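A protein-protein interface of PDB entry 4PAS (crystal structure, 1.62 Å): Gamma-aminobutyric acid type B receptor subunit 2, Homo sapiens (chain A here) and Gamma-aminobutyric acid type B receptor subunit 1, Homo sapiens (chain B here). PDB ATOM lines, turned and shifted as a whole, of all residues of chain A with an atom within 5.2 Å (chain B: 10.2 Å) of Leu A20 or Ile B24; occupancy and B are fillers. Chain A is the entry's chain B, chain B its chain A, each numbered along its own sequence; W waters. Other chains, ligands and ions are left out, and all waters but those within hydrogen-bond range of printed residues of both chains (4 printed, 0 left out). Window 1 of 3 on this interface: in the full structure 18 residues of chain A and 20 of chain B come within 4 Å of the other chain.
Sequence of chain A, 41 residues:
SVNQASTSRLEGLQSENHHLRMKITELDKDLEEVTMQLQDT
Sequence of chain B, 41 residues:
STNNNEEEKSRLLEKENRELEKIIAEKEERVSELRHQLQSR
The side-chain carboxylate of Glu B16 lies within hydrogen-bond range of the side-chain amide nitrogen of Asn A17 (2.9 Å). The guanidinium group (NH2) of Arg A21 lies within salt-bridge range of the side-chain carboxylate (OE2) of Glu B16, at 2.8 Å. The side-chain carboxylate (OE1) of Glu A16 sits at hydrogen-bond distance from the side-chain amide nitrogen (ND2) of Asn B17. The side-chain amide oxygen (OD1) of Asn B17 lies within hydrogen-bond range of the side-chain amide nitrogen (ND2) of Asn A17, 2.8 Å away. The guanidinium group (NH2) of Arg B18 is in salt-bridge range of the side-chain carboxylate (OE2) of Glu A16 (3.3 Å).
The backbone carbonyl oxygen (O) of Leu B13 sits close to the side-chain amide oxygen (OD1) of Asn B17 (3.4 Å). The guanidinium group of Arg B18 is in salt-bridge range of the side-chain carboxylate of Glu B14 (2.5 Å). NH2 of Arg B18 is in salt-bridge range of OE2 of Glu B21 (2.7 Å). The side-chain amide oxygen of Asn A17 lies within hydrogen-bond range of the guanidinium group of Arg A21 (2.9 Å).
Leu B20 touches Asn A17. Leu A20 touches Asn B17. CD2 of Leu A20 touches CG of Glu B21, at 3.97 Å. Leu A20 touches Ile B24 (O to CD1, 3.6 Å). CB of Lys A23 touches CD1 of Ile B24, at 3.98 Å. Leu B20 touches Ile A24 (CD2 to CD1, 3.8 Å). CD1 of Ile A24 touches CG2 of Ile B23 (3.99 Å). Ile A24 touches Ile B24 (CG1 to CG1, 3.6 Å). Lys B27 touches Ile A24 (CE to CG2, 3.9 Å). Leu A27 touches Ile B24 (CD1 to CG2, 3.7 Å).
Of chain B, only Asn B17, Glu B21 and Ile B24 come within 4 Å of Leu A20. Of the printed residues of chain B, Leu A27 touches Ile B24 (3.7 Å) and Glu B28 (3.3 Å). Lys B15 touches none of the printed residues of chain A. Lys B22 touches none of the printed residues of chain A. Of the printed residues of chain A, Ile B24 touches Leu A20 (3.6 Å), Lys A23 (3.98 Å), Ile A24 (3.6 Å) and Leu A27 (3.7 Å). Of the printed residues of chain A, Glu B28 touches Leu A27. The nearest printed residue of chain A that does not touch Ile B24 is Arg A21 (5.4 Å).
Of the 10 printed residues of chain A, 7 touch a printed residue of chain B. Printed residues of chain A that touch a printed residue of chain B: Glu A16, Asn A17, Leu A20, Arg A21, Lys A23, Ile A24 and Leu A27. Hydrophobic or aromatic side chains of chain A within 4 Å of the printed part of chain B: Leu A20, Ile A24 and Leu A27. Hydrophobic or aromatic side chains of chain B within 4 Å of the printed part of chain A: Leu B13, Leu B20, Ile B23 and Ile B24. Among the printed residues, Asp or Glu carboxylates within 4 Å of a Lys or Arg side-chain nitrogen of the other chain: Glu A16 with Arg B18 and Arg A21 with Glu B16.
Water W4 lies within hydrogen-bond range of OE1 of Glu B14 (2.6 Å), OE1 of Glu A16 (2.7 Å) and NH1 of Arg B18 (2.8 Å). Water W1 bridges the guanidinium group (NH2) of Arg B18 and the side-chain carboxylate (OE2) of Glu A16. Water W2 bridges OE2 of Glu A16 and OE2 of Glu B21. Water W3 lies within hydrogen-bond range of the side-chain carboxylate (OE2) of Glu B16 (3.0 Å) and the side-chain amide oxygen (OD1) of Asn A17 (3.3 Å).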
ATOM      1  N   GLU A  16      10.980  11.634 -22.045  1.00  0.00           N
ATOM      2  CA  GLU A  16      10.246  12.893 -22.048  1.00  0.00           C
ATOM      3  C   GLU A  16      11.082  14.002 -22.686  1.00  0.00           C
ATOM      4  O   GLU A  16      10.576  14.803 -23.469  1.00  0.00           O
ATOM      5  CB  GLU A  16       9.858  13.281 -20.617  1.00  0.00           C
ATOM      6  CG  GLU A  16       9.053  14.578 -20.541  1.00  0.00           C
ATOM      7  CD  GLU A  16       8.682  14.968 -19.131  1.00  0.00           C
ATOM      8  OE1 GLU A  16       9.516  14.797 -18.211  1.00  0.00           O
ATOM      9  OE2 GLU A  16       7.551  15.471 -18.933  1.00  0.00           O
ATOM     10  N   ASN A  17      12.371  14.030 -22.359  1.00  0.00           N
ATOM     11  CA  ASN A  17      13.277  15.039 -22.904  1.00  0.00           C
ATOM     12  C   ASN A  17      13.288  14.978 -24.429  1.00  0.00           C
ATOM     13  O   ASN A  17      13.235  16.009 -25.099  1.00  0.00           O
ATOM     14  CB  ASN A  17      14.693  14.824 -22.354  1.00  0.00           C
ATOM     15  CG  ASN A  17      15.630  15.961 -22.701  1.00  0.00           C
ATOM     16  OD1 ASN A  17      16.351  15.901 -23.702  1.00  0.00           O
ATOM     17  ND2 ASN A  17      15.624  17.009 -21.883  1.00  0.00           N
ATOM     18  N   HIS A  18      13.342  13.768 -24.980  1.00  0.00           N
ATOM     19  CA  HIS A  18      13.342  13.615 -26.430  1.00  0.00           C
ATOM     20  C   HIS A  18      12.031  14.080 -27.049  1.00  0.00           C
ATOM     21  O   HIS A  18      12.028  14.751 -28.089  1.00  0.00           O
ATOM     22  CB  HIS A  18      13.607  12.161 -26.813  1.00  0.00           C
ATOM     23  CG  HIS A  18      13.610  11.931 -28.292  1.00  0.00           C
ATOM     24  ND1 HIS A  18      14.431  12.631 -29.150  1.00  0.00           N
ATOM     25  CD2 HIS A  18      12.893  11.080 -29.066  1.00  0.00           C
ATOM     26  CE1 HIS A  18      14.217  12.227 -30.390  1.00  0.00           C
ATOM     27  NE2 HIS A  18      13.291  11.286 -30.366  1.00  0.00           N
ATOM     28  N   HIS A  19      10.919  13.725 -26.413  1.00  0.00           N
ATOM     29  CA  HIS A  19       9.606  14.176 -26.862  1.00  0.00           C
ATOM     30  C   HIS A  19       9.571  15.703 -26.971  1.00  0.00           C
ATOM     31  O   HIS A  19       9.128  16.263 -27.981  1.00  0.00           O
ATOM     32  CB  HIS A  19       8.532  13.684 -25.890  1.00  0.00           C
ATOM     33  CG  HIS A  19       7.188  14.306 -26.099  1.00  0.00           C
ATOM     34  ND1 HIS A  19       6.463  14.145 -27.261  1.00  0.00           N
ATOM     35  CD2 HIS A  19       6.426  15.075 -25.283  1.00  0.00           C
ATOM     36  CE1 HIS A  19       5.315  14.792 -27.154  1.00  0.00           C
ATOM     37  NE2 HIS A  19       5.268  15.363 -25.963  1.00  0.00           N
ATOM     38  N   LEU A  20      10.057  16.375 -25.932  1.00  0.00           N
ATOM     39  CA  LEU A  20      10.041  17.838 -25.888  1.00  0.00           C
ATOM     40  C   LEU A  20      10.960  18.447 -26.935  1.00  0.00           C
ATOM     41  O   LEU A  20      10.617  19.455 -27.566  1.00  0.00           O
ATOM     42  CB  LEU A  20      10.419  18.331 -24.483  1.00  0.00           C
ATOM     43  CG  LEU A  20       9.443  17.889 -23.383  1.00  0.00           C
ATOM     44  CD1 LEU A  20       9.985  18.266 -22.010  1.00  0.00           C
ATOM     45  CD2 LEU A  20       8.057  18.504 -23.590  1.00  0.00           C
ATOM     46  N   ARG A  21      12.117  17.835 -27.139  1.00  0.00           N
ATOM     47  CA  ARG A  21      13.056  18.357 -28.135  1.00  0.00           C
ATOM     48  C   ARG A  21      12.534  18.176 -29.552  1.00  0.00           C
ATOM     49  O   ARG A  21      12.779  19.016 -30.420  1.00  0.00           O
ATOM     50  CB  ARG A  21      14.430  17.715 -27.955  1.00  0.00           C
ATOM     51  CG  ARG A  21      15.139  18.225 -26.703  1.00  0.00           C
ATOM     52  CD  ARG A  21      16.478  17.553 -26.489  1.00  0.00           C
ATOM     53  NE  ARG A  21      17.206  18.163 -25.381  1.00  0.00           N
ATOM     54  CZ  ARG A  21      17.791  19.357 -25.440  1.00  0.00           C
ATOM     55  NH1 ARG A  21      17.737  20.075 -26.556  1.00  0.00           N
ATOM     56  NH2 ARG A  21      18.427  19.843 -24.380  1.00  0.00           N
ATOM     57  N   MET A  22      11.820  17.083 -29.792  1.00  0.00           N
ATOM     58  CA  MET A  22      11.206  16.861 -31.099  1.00  0.00           C
ATOM     59  C   MET A  22      10.108  17.893 -31.337  1.00  0.00           C
ATOM     60  O   MET A  22       9.946  18.376 -32.448  1.00  0.00           O
ATOM     61  CB  MET A  22      10.662  15.436 -31.208  1.00  0.00           C
ATOM     62  CG  MET A  22      11.746  14.370 -31.258  1.00  0.00           C
ATOM     63  SD  MET A  22      12.757  14.405 -32.766  1.00  0.00           S
ATOM     64  CE  MET A  22      11.725  13.489 -33.898  1.00  0.00           C
ATOM     65  N   LYS A  23       9.368  18.237 -30.286  1.00  0.00           N
ATOM     66  CA  LYS A  23       8.332  19.268 -30.388  1.00  0.00           C
ATOM     67  C   LYS A  23       8.951  20.616 -30.720  1.00  0.00           C
ATOM     68  O   LYS A  23       8.393  21.394 -31.502  1.00  0.00           O
ATOM     69  CB  LYS A  23       7.541  19.377 -29.083  1.00  0.00           C
ATOM     70  CG  LYS A  23       6.596  18.214 -28.838  1.00  0.00           C
ATOM     71  CD  LYS A  23       5.849  18.346 -27.516  1.00  0.00           C
ATOM     72  CE  LYS A  23       4.897  19.528 -27.519  1.00  0.00           C
ATOM     73  NZ  LYS A  23       3.785  19.322 -26.531  1.00  0.00           N
ATOM     74  N   ILE A  24      10.111  20.900 -30.137  1.00  0.00           N
ATOM     75  CA  ILE A  24      10.787  22.163 -30.426  1.00  0.00           C
ATOM     76  C   ILE A  24      11.225  22.228 -31.883  1.00  0.00           C
ATOM     77  O   ILE A  24      11.104  23.263 -32.525  1.00  0.00           O
ATOM     78  CB  ILE A  24      11.980  22.396 -29.475  1.00  0.00           C
ATOM     79  CG1 ILE A  24      11.448  22.716 -28.076  1.00  0.00           C
ATOM     80  CG2 ILE A  24      12.862  23.550 -29.981  1.00  0.00           C
ATOM     81  CD1 ILE A  24      12.517  22.800 -26.986  1.00  0.00           C
ATOM     82  N   LEU A  27       8.217  23.148 -33.792  1.00  0.00           N
ATOM     83  CA  LEU A  27       7.849  24.551 -33.588  1.00  0.00           C
ATOM     84  C   LEU A  27       8.775  25.513 -34.306  1.00  0.00           C
ATOM     85  O   LEU A  27       8.327  26.546 -34.810  1.00  0.00           O
ATOM     86  CB  LEU A  27       7.806  24.888 -32.095  1.00  0.00           C
ATOM     87  CG  LEU A  27       6.585  24.274 -31.425  1.00  0.00           C
ATOM     88  CD1 LEU A  27       6.679  24.388 -29.914  1.00  0.00           C
ATOM     89  CD2 LEU A  27       5.316  24.966 -31.951  1.00  0.00           C
ATOM     90  N   LEU B  13      17.557  16.619 -14.798  1.00  0.00           N
ATOM     91  CA  LEU B  13      16.808  16.413 -16.040  1.00  0.00           C
ATOM     92  C   LEU B  13      15.360  16.861 -15.887  1.00  0.00           C
ATOM     93  O   LEU B  13      14.757  17.373 -16.832  1.00  0.00           O
ATOM     94  CB  LEU B  13      16.886  14.952 -16.498  1.00  0.00           C
ATOM     95  CG  LEU B  13      16.424  14.675 -17.936  1.00  0.00           C
ATOM     96  CD1 LEU B  13      17.096  15.618 -18.933  1.00  0.00           C
ATOM     97  CD2 LEU B  13      16.724  13.235 -18.290  1.00  0.00           C
ATOM     98  N   GLU B  14      14.801  16.665 -14.701  1.00  0.00           N
ATOM     99  CA  GLU B  14      13.451  17.141 -14.414  1.00  0.00           C
ATOM    100  C   GLU B  14      13.394  18.655 -14.620  1.00  0.00           C
ATOM    101  O   GLU B  14      12.460  19.167 -15.241  1.00  0.00           O
ATOM    102  CB  GLU B  14      13.068  16.780 -12.979  1.00  0.00           C
ATOM    103  CG  GLU B  14      11.781  17.419 -12.475  1.00  0.00           C
ATOM    104  CD  GLU B  14      10.537  16.856 -13.125  1.00  0.00           C
ATOM    105  OE1 GLU B  14      10.583  15.724 -13.650  1.00  0.00           O
ATOM    106  OE2 GLU B  14       9.499  17.553 -13.097  1.00  0.00           O
ATOM    107  N   LYS B  15      14.399  19.369 -14.114  1.00  0.00           N
ATOM    108  CA  LYS B  15      14.444  20.825 -14.285  1.00  0.00           C
ATOM    109  C   LYS B  15      14.640  21.224 -15.751  1.00  0.00           C
ATOM    110  O   LYS B  15      14.062  22.213 -16.208  1.00  0.00           O
ATOM    111  CB  LYS B  15      15.542  21.449 -13.409  1.00  0.00           C
ATOM    112  CG  LYS B  15      15.263  21.367 -11.896  1.00  0.00           C
ATOM    113  CD  LYS B  15      13.939  22.054 -11.533  1.00  0.00           C
ATOM    114  CE  LYS B  15      13.706  22.121 -10.031  1.00  0.00           C
ATOM    115  NZ  LYS B  15      13.660  20.777  -9.393  1.00  0.00           N
ATOM    116  N   GLU B  16      15.460  20.466 -16.479  1.00  0.00           N
ATOM    117  CA  GLU B  16      15.654  20.731 -17.901  1.00  0.00           C
ATOM    118  C   GLU B  16      14.340  20.567 -18.652  1.00  0.00           C
ATOM    119  O   GLU B  16      13.964  21.410 -19.465  1.00  0.00           O
ATOM    120  CB  GLU B  16      16.721  19.814 -18.511  1.00  0.00           C
ATOM    121  CG  GLU B  16      16.874  20.038 -20.026  1.00  0.00           C
ATOM    122  CD  GLU B  16      18.015  19.257 -20.662  1.00  0.00           C
ATOM    123  OE1 GLU B  16      19.083  19.120 -20.029  1.00  0.00           O
ATOM    124  OE2 GLU B  16      17.847  18.796 -21.803  1.00  0.00           O
ATOM    125  N   ASN B  17      13.629  19.481 -18.376  1.00  0.00           N
ATOM    126  CA  ASN B  17      12.364  19.238 -19.058  1.00  0.00           C
ATOM    127  C   ASN B  17      11.356  20.344 -18.771  1.00  0.00           C
ATOM    128  O   ASN B  17      10.624  20.779 -19.660  1.00  0.00           O
ATOM    129  CB  ASN B  17      11.799  17.874 -18.644  1.00  0.00           C
ATOM    130  CG  ASN B  17      12.602  16.719 -19.208  1.00  0.00           C
ATOM    131  OD1 ASN B  17      13.544  16.923 -19.983  1.00  0.00           O
ATOM    132  ND2 ASN B  17      12.227  15.503 -18.847  1.00  0.00           N
ATOM    133  N   ARG B  18      11.323  20.813 -17.527  1.00  0.00           N
ATOM    134  CA  ARG B  18      10.423  21.906 -17.170  1.00  0.00           C
ATOM    135  C   ARG B  18      10.761  23.150 -17.981  1.00  0.00           C
ATOM    136  O   ARG B  18       9.865  23.858 -18.456  1.00  0.00           O
ATOM    137  CB  ARG B  18      10.528  22.228 -15.676  1.00  0.00           C
ATOM    138  CG  ARG B  18       9.965  21.169 -14.739  1.00  0.00           C
ATOM    139  CD  ARG B  18       8.439  21.001 -14.836  1.00  0.00           C
ATOM    140  NE  ARG B  18       8.008  20.169 -15.966  1.00  0.00           N
ATOM    141  CZ  ARG B  18       8.448  18.935 -16.215  1.00  0.00           C
ATOM    142  NH1 ARG B  18       9.359  18.371 -15.432  1.00  0.00           N
ATOM    143  NH2 ARG B  18       7.981  18.263 -17.263  1.00  0.00           N
ATOM    144  N   GLU B  19      12.057  23.418 -18.142  1.00  0.00           N
ATOM    145  CA  GLU B  19      12.487  24.589 -18.907  1.00  0.00           C
ATOM    146  C   GLU B  19      12.141  24.424 -20.384  1.00  0.00           C
ATOM    147  O   GLU B  19      11.734  25.385 -21.038  1.00  0.00           O
ATOM    148  CB  GLU B  19      13.989  24.833 -18.737  1.00  0.00           C
ATOM    149  CG  GLU B  19      14.424  26.255 -19.088  1.00  0.00           C
ATOM    150  CD  GLU B  19      13.739  27.316 -18.227  1.00  0.00           C
ATOM    151  OE1 GLU B  19      13.286  26.993 -17.103  1.00  0.00           O
ATOM    152  OE2 GLU B  19      13.666  28.477 -18.671  1.00  0.00           O
ATOM    153  N   LEU B  20      12.281  23.209 -20.905  1.00  0.00           N
ATOM    154  CA  LEU B  20      11.923  22.944 -22.301  1.00  0.00           C
ATOM    155  C   LEU B  20      10.426  23.150 -22.515  1.00  0.00           C
ATOM    156  O   LEU B  20      10.013  23.615 -23.582  1.00  0.00           O
ATOM    157  CB  LEU B  20      12.344  21.530 -22.720  1.00  0.00           C
ATOM    158  CG  LEU B  20      13.851  21.246 -22.811  1.00  0.00           C
ATOM    159  CD1 LEU B  20      14.099  19.786 -23.162  1.00  0.00           C
ATOM    160  CD2 LEU B  20      14.509  22.148 -23.849  1.00  0.00           C
ATOM    161  N   GLU B  21       9.612  22.830 -21.506  1.00  0.00           N
ATOM    162  CA  GLU B  21       8.167  23.061 -21.614  1.00  0.00           C
ATOM    163  C   GLU B  21       7.873  24.552 -21.681  1.00  0.00           C
ATOM    164  O   GLU B  21       6.971  24.983 -22.404  1.00  0.00           O
ATOM    165  CB  GLU B  21       7.407  22.426 -20.444  1.00  0.00           C
ATOM    166  CG  GLU B  21       7.294  20.919 -20.531  1.00  0.00           C
ATOM    167  CD  GLU B  21       6.178  20.366 -19.670  1.00  0.00           C
ATOM    168  OE1 GLU B  21       5.139  21.055 -19.507  1.00  0.00           O
ATOM    169  OE2 GLU B  21       6.332  19.236 -19.171  1.00  0.00           O
ATOM    170  N   LYS B  22       8.635  25.339 -20.928  1.00  0.00           N
ATOM    171  CA  LYS B  22       8.483  26.796 -20.959  1.00  0.00           C
ATOM    172  C   LYS B  22       8.863  27.335 -22.338  1.00  0.00           C
ATOM    173  O   LYS B  22       8.186  28.214 -22.876  1.00  0.00           O
ATOM    174  CB  LYS B  22       9.338  27.461 -19.870  1.00  0.00           C
ATOM    175  CG  LYS B  22       8.845  27.213 -18.458  1.00  0.00           C
ATOM    176  CD  LYS B  22       9.760  27.865 -17.426  1.00  0.00           C
ATOM    177  CE  LYS B  22       9.316  27.533 -16.005  1.00  0.00           C
ATOM    178  NZ  LYS B  22       7.827  27.615 -15.839  1.00  0.00           N
ATOM    179  N   ILE B  23       9.935  26.793 -22.913  1.00  0.00           N
ATOM    180  CA  ILE B  23      10.387  27.194 -24.244  1.00  0.00           C
ATOM    181  C   ILE B  23       9.314  26.846 -25.278  1.00  0.00           C
ATOM    182  O   ILE B  23       9.028  27.634 -26.179  1.00  0.00           O
ATOM    183  CB  ILE B  23      11.736  26.519 -24.606  1.00  0.00           C
ATOM    184  CG1 ILE B  23      12.858  27.124 -23.757  1.00  0.00           C
ATOM    185  CG2 ILE B  23      12.041  26.663 -26.100  1.00  0.00           C
ATOM    186  CD1 ILE B  23      14.176  26.350 -23.813  1.00  0.00           C
ATOM    187  N   ILE B  24       8.719  25.666 -25.133  1.00  0.00           N
ATOM    188  CA  ILE B  24       7.658  25.229 -26.033  1.00  0.00           C
ATOM    189  C   ILE B  24       6.458  26.178 -25.954  1.00  0.00           C
ATOM    190  O   ILE B  24       5.911  26.584 -26.984  1.00  0.00           O
ATOM    191  CB  ILE B  24       7.255  23.769 -25.731  1.00  0.00           C
ATOM    192  CG1 ILE B  24       8.359  22.830 -26.233  1.00  0.00           C
ATOM    193  CG2 ILE B  24       5.934  23.420 -26.385  1.00  0.00           C
ATOM    194  CD1 ILE B  24       8.248  21.399 -25.728  1.00  0.00           C
ATOM    195  N   ALA B  25       6.061  26.543 -24.738  1.00  0.00           N
ATOM    196  CA  ALA B  25       4.938  27.469 -24.566  1.00  0.00           C
ATOM    197  C   ALA B  25       5.267  28.828 -25.191  1.00  0.00           C
ATOM    198  O   ALA B  25       4.416  29.455 -25.838  1.00  0.00           O
ATOM    199  CB  ALA B  25       4.595  27.626 -23.099  1.00  0.00           C
ATOM    200  N   GLU B  26       6.506  29.275 -25.016  1.00  0.00           N
ATOM    201  CA  GLU B  26       6.929  30.551 -25.584  1.00  0.00           C
ATOM    202  C   GLU B  26       6.883  30.524 -27.104  1.00  0.00           C
ATOM    203  O   GLU B  26       6.432  31.486 -27.737  1.00  0.00           O
ATOM    204  CB  GLU B  26       8.331  30.910 -25.099  1.00  0.00           C
ATOM    205  CG  GLU B  26       8.351  31.353 -23.653  1.00  0.00           C
ATOM    206  CD  GLU B  26       9.752  31.433 -23.090  1.00  0.00           C
ATOM    207  OE1 GLU B  26      10.716  31.393 -23.881  1.00  0.00           O
ATOM    208  OE2 GLU B  26       9.879  31.529 -21.853  1.00  0.00           O
ATOM    209  N   LYS B  27       7.329  29.418 -27.690  1.00  0.00           N
ATOM    210  CA  LYS B  27       7.346  29.298 -29.145  1.00  0.00           C
ATOM    211  C   LYS B  27       5.936  29.181 -29.718  1.00  0.00           C
ATOM    212  O   LYS B  27       5.646  29.771 -30.756  1.00  0.00           O
ATOM    213  CB  LYS B  27       8.206  28.110 -29.588  1.00  0.00           C
ATOM    214  CG  LYS B  27       9.702  28.337 -29.386  1.00  0.00           C
ATOM    215  CD  LYS B  27      10.508  27.107 -29.796  1.00  0.00           C
ATOM    216  CE  LYS B  27      12.012  27.314 -29.610  1.00  0.00           C
ATOM    217  NZ  LYS B  27      12.563  28.372 -30.513  1.00  0.00           N
ATOM    218  N   GLU B  28       5.056  28.440 -29.044  1.00  0.00           N
ATOM    219  CA  GLU B  28       3.664  28.338 -29.503  1.00  0.00           C
ATOM    220  C   GLU B  28       2.984  29.697 -29.433  1.00  0.00           C
ATOM    221  O   GLU B  28       2.230  30.066 -30.330  1.00  0.00           O
ATOM    222  CB  GLU B  28       2.865  27.323 -28.672  1.00  0.00           C
ATOM    223  CG  GLU B  28       3.216  25.868 -28.919  1.00  0.00           C
ATOM    224  CD  GLU B  28       2.543  25.269 -30.151  1.00  0.00           C
ATOM    225  OE1 GLU B  28       2.184  26.010 -31.096  1.00  0.00           O
ATOM    226  OE2 GLU B  28       2.400  24.033 -30.187  1.00  0.00           O
ATOM    227  N   GLU B  29       3.248  30.448 -28.366  1.00  0.00           N
ATOM    228  CA  GLU B  29       2.650  31.777 -28.240  1.00  0.00           C
ATOM    229  C   GLU B  29       3.166  32.699 -29.345  1.00  0.00           C
ATOM    230  O   GLU B  29       2.402  33.484 -29.905  1.00  0.00           O
ATOM    231  CB  GLU B  29       2.915  32.360 -26.851  1.00  0.00           C
ATOM    232  CG  GLU B  29       2.284  33.727 -26.593  1.00  0.00           C
ATOM    233  CD  GLU B  29       0.796  33.793 -26.912  1.00  0.00           C
ATOM    234  OE1 GLU B  29       0.075  32.787 -26.724  1.00  0.00           O
ATOM    235  OE2 GLU B  29       0.334  34.872 -27.339  1.00  0.00           O
ATOM    236  N   ARG B  30       4.453  32.592 -29.675  1.00  0.00           N
ATOM    237  CA  ARG B  30       5.011  33.384 -30.769  1.00  0.00           C
ATOM    238  C   ARG B  30       4.355  33.031 -32.107  1.00  0.00           C
ATOM    239  O   ARG B  30       4.037  33.923 -32.891  1.00  0.00           O
ATOM    240  CB  ARG B  30       6.532  33.220 -30.859  1.00  0.00           C
ATOM    241  CG  ARG B  30       7.186  34.134 -31.882  1.00  0.00           C
ATOM    242  CD  ARG B  30       6.808  35.576 -31.619  1.00  0.00           C
ATOM    243  NE  ARG B  30       7.340  36.479 -32.629  1.00  0.00           N
ATOM    244  CZ  ARG B  30       6.914  37.721 -32.802  1.00  0.00           C
ATOM    245  NH1 ARG B  30       5.943  38.204 -32.030  1.00  0.00           N
ATOM    246  NH2 ARG B  30       7.456  38.478 -33.747  1.00  0.00           N
ATOM    247  N   VAL B  31       4.144  31.738 -32.363  1.00  0.00           N
ATOM    248  CA  VAL B  31       3.473  31.319 -33.602  1.00  0.00           C
ATOM    249  C   VAL B  31       2.062  31.896 -33.626  1.00  0.00           C
ATOM    250  O   VAL B  31       1.569  32.325 -34.672  1.00  0.00           O
ATOM    251  CB  VAL B  31       3.408  29.780 -33.733  1.00  0.00           C
ATOM    252  CG1 VAL B  31       2.471  29.364 -34.883  1.00  0.00           C
ATOM    253  CG2 VAL B  31       4.796  29.219 -33.985  1.00  0.00           C
ATOM    254  N   SER B  32       1.414  31.901 -32.465  1.00  0.00           N
ATOM    255  CA  SER B  32       0.066  32.464 -32.346  1.00  0.00           C
ATOM    256  C   SER B  32       0.066  33.960 -32.637  1.00  0.00           C
ATOM    257  O   SER B  32      -0.814  34.461 -33.338  1.00  0.00           O
ATOM    258  CB  SER B  32      -0.504  32.189 -30.955  1.00  0.00           C
ATOM    259  OG  SER B  32      -1.796  32.758 -30.830  1.00  0.00           O
HETATM  260  O   HOH W   1       6.164  16.356 -16.695  1.00  0.00           O
HETATM  261  O   HOH W   2       6.217  16.879 -20.821  1.00  0.00           O
HETATM  262  O   HOH W   3      19.362  16.223 -22.366  1.00  0.00           O
HETATM  263  O   HOH W   4       8.953  15.642 -15.708  1.00  0.00           O
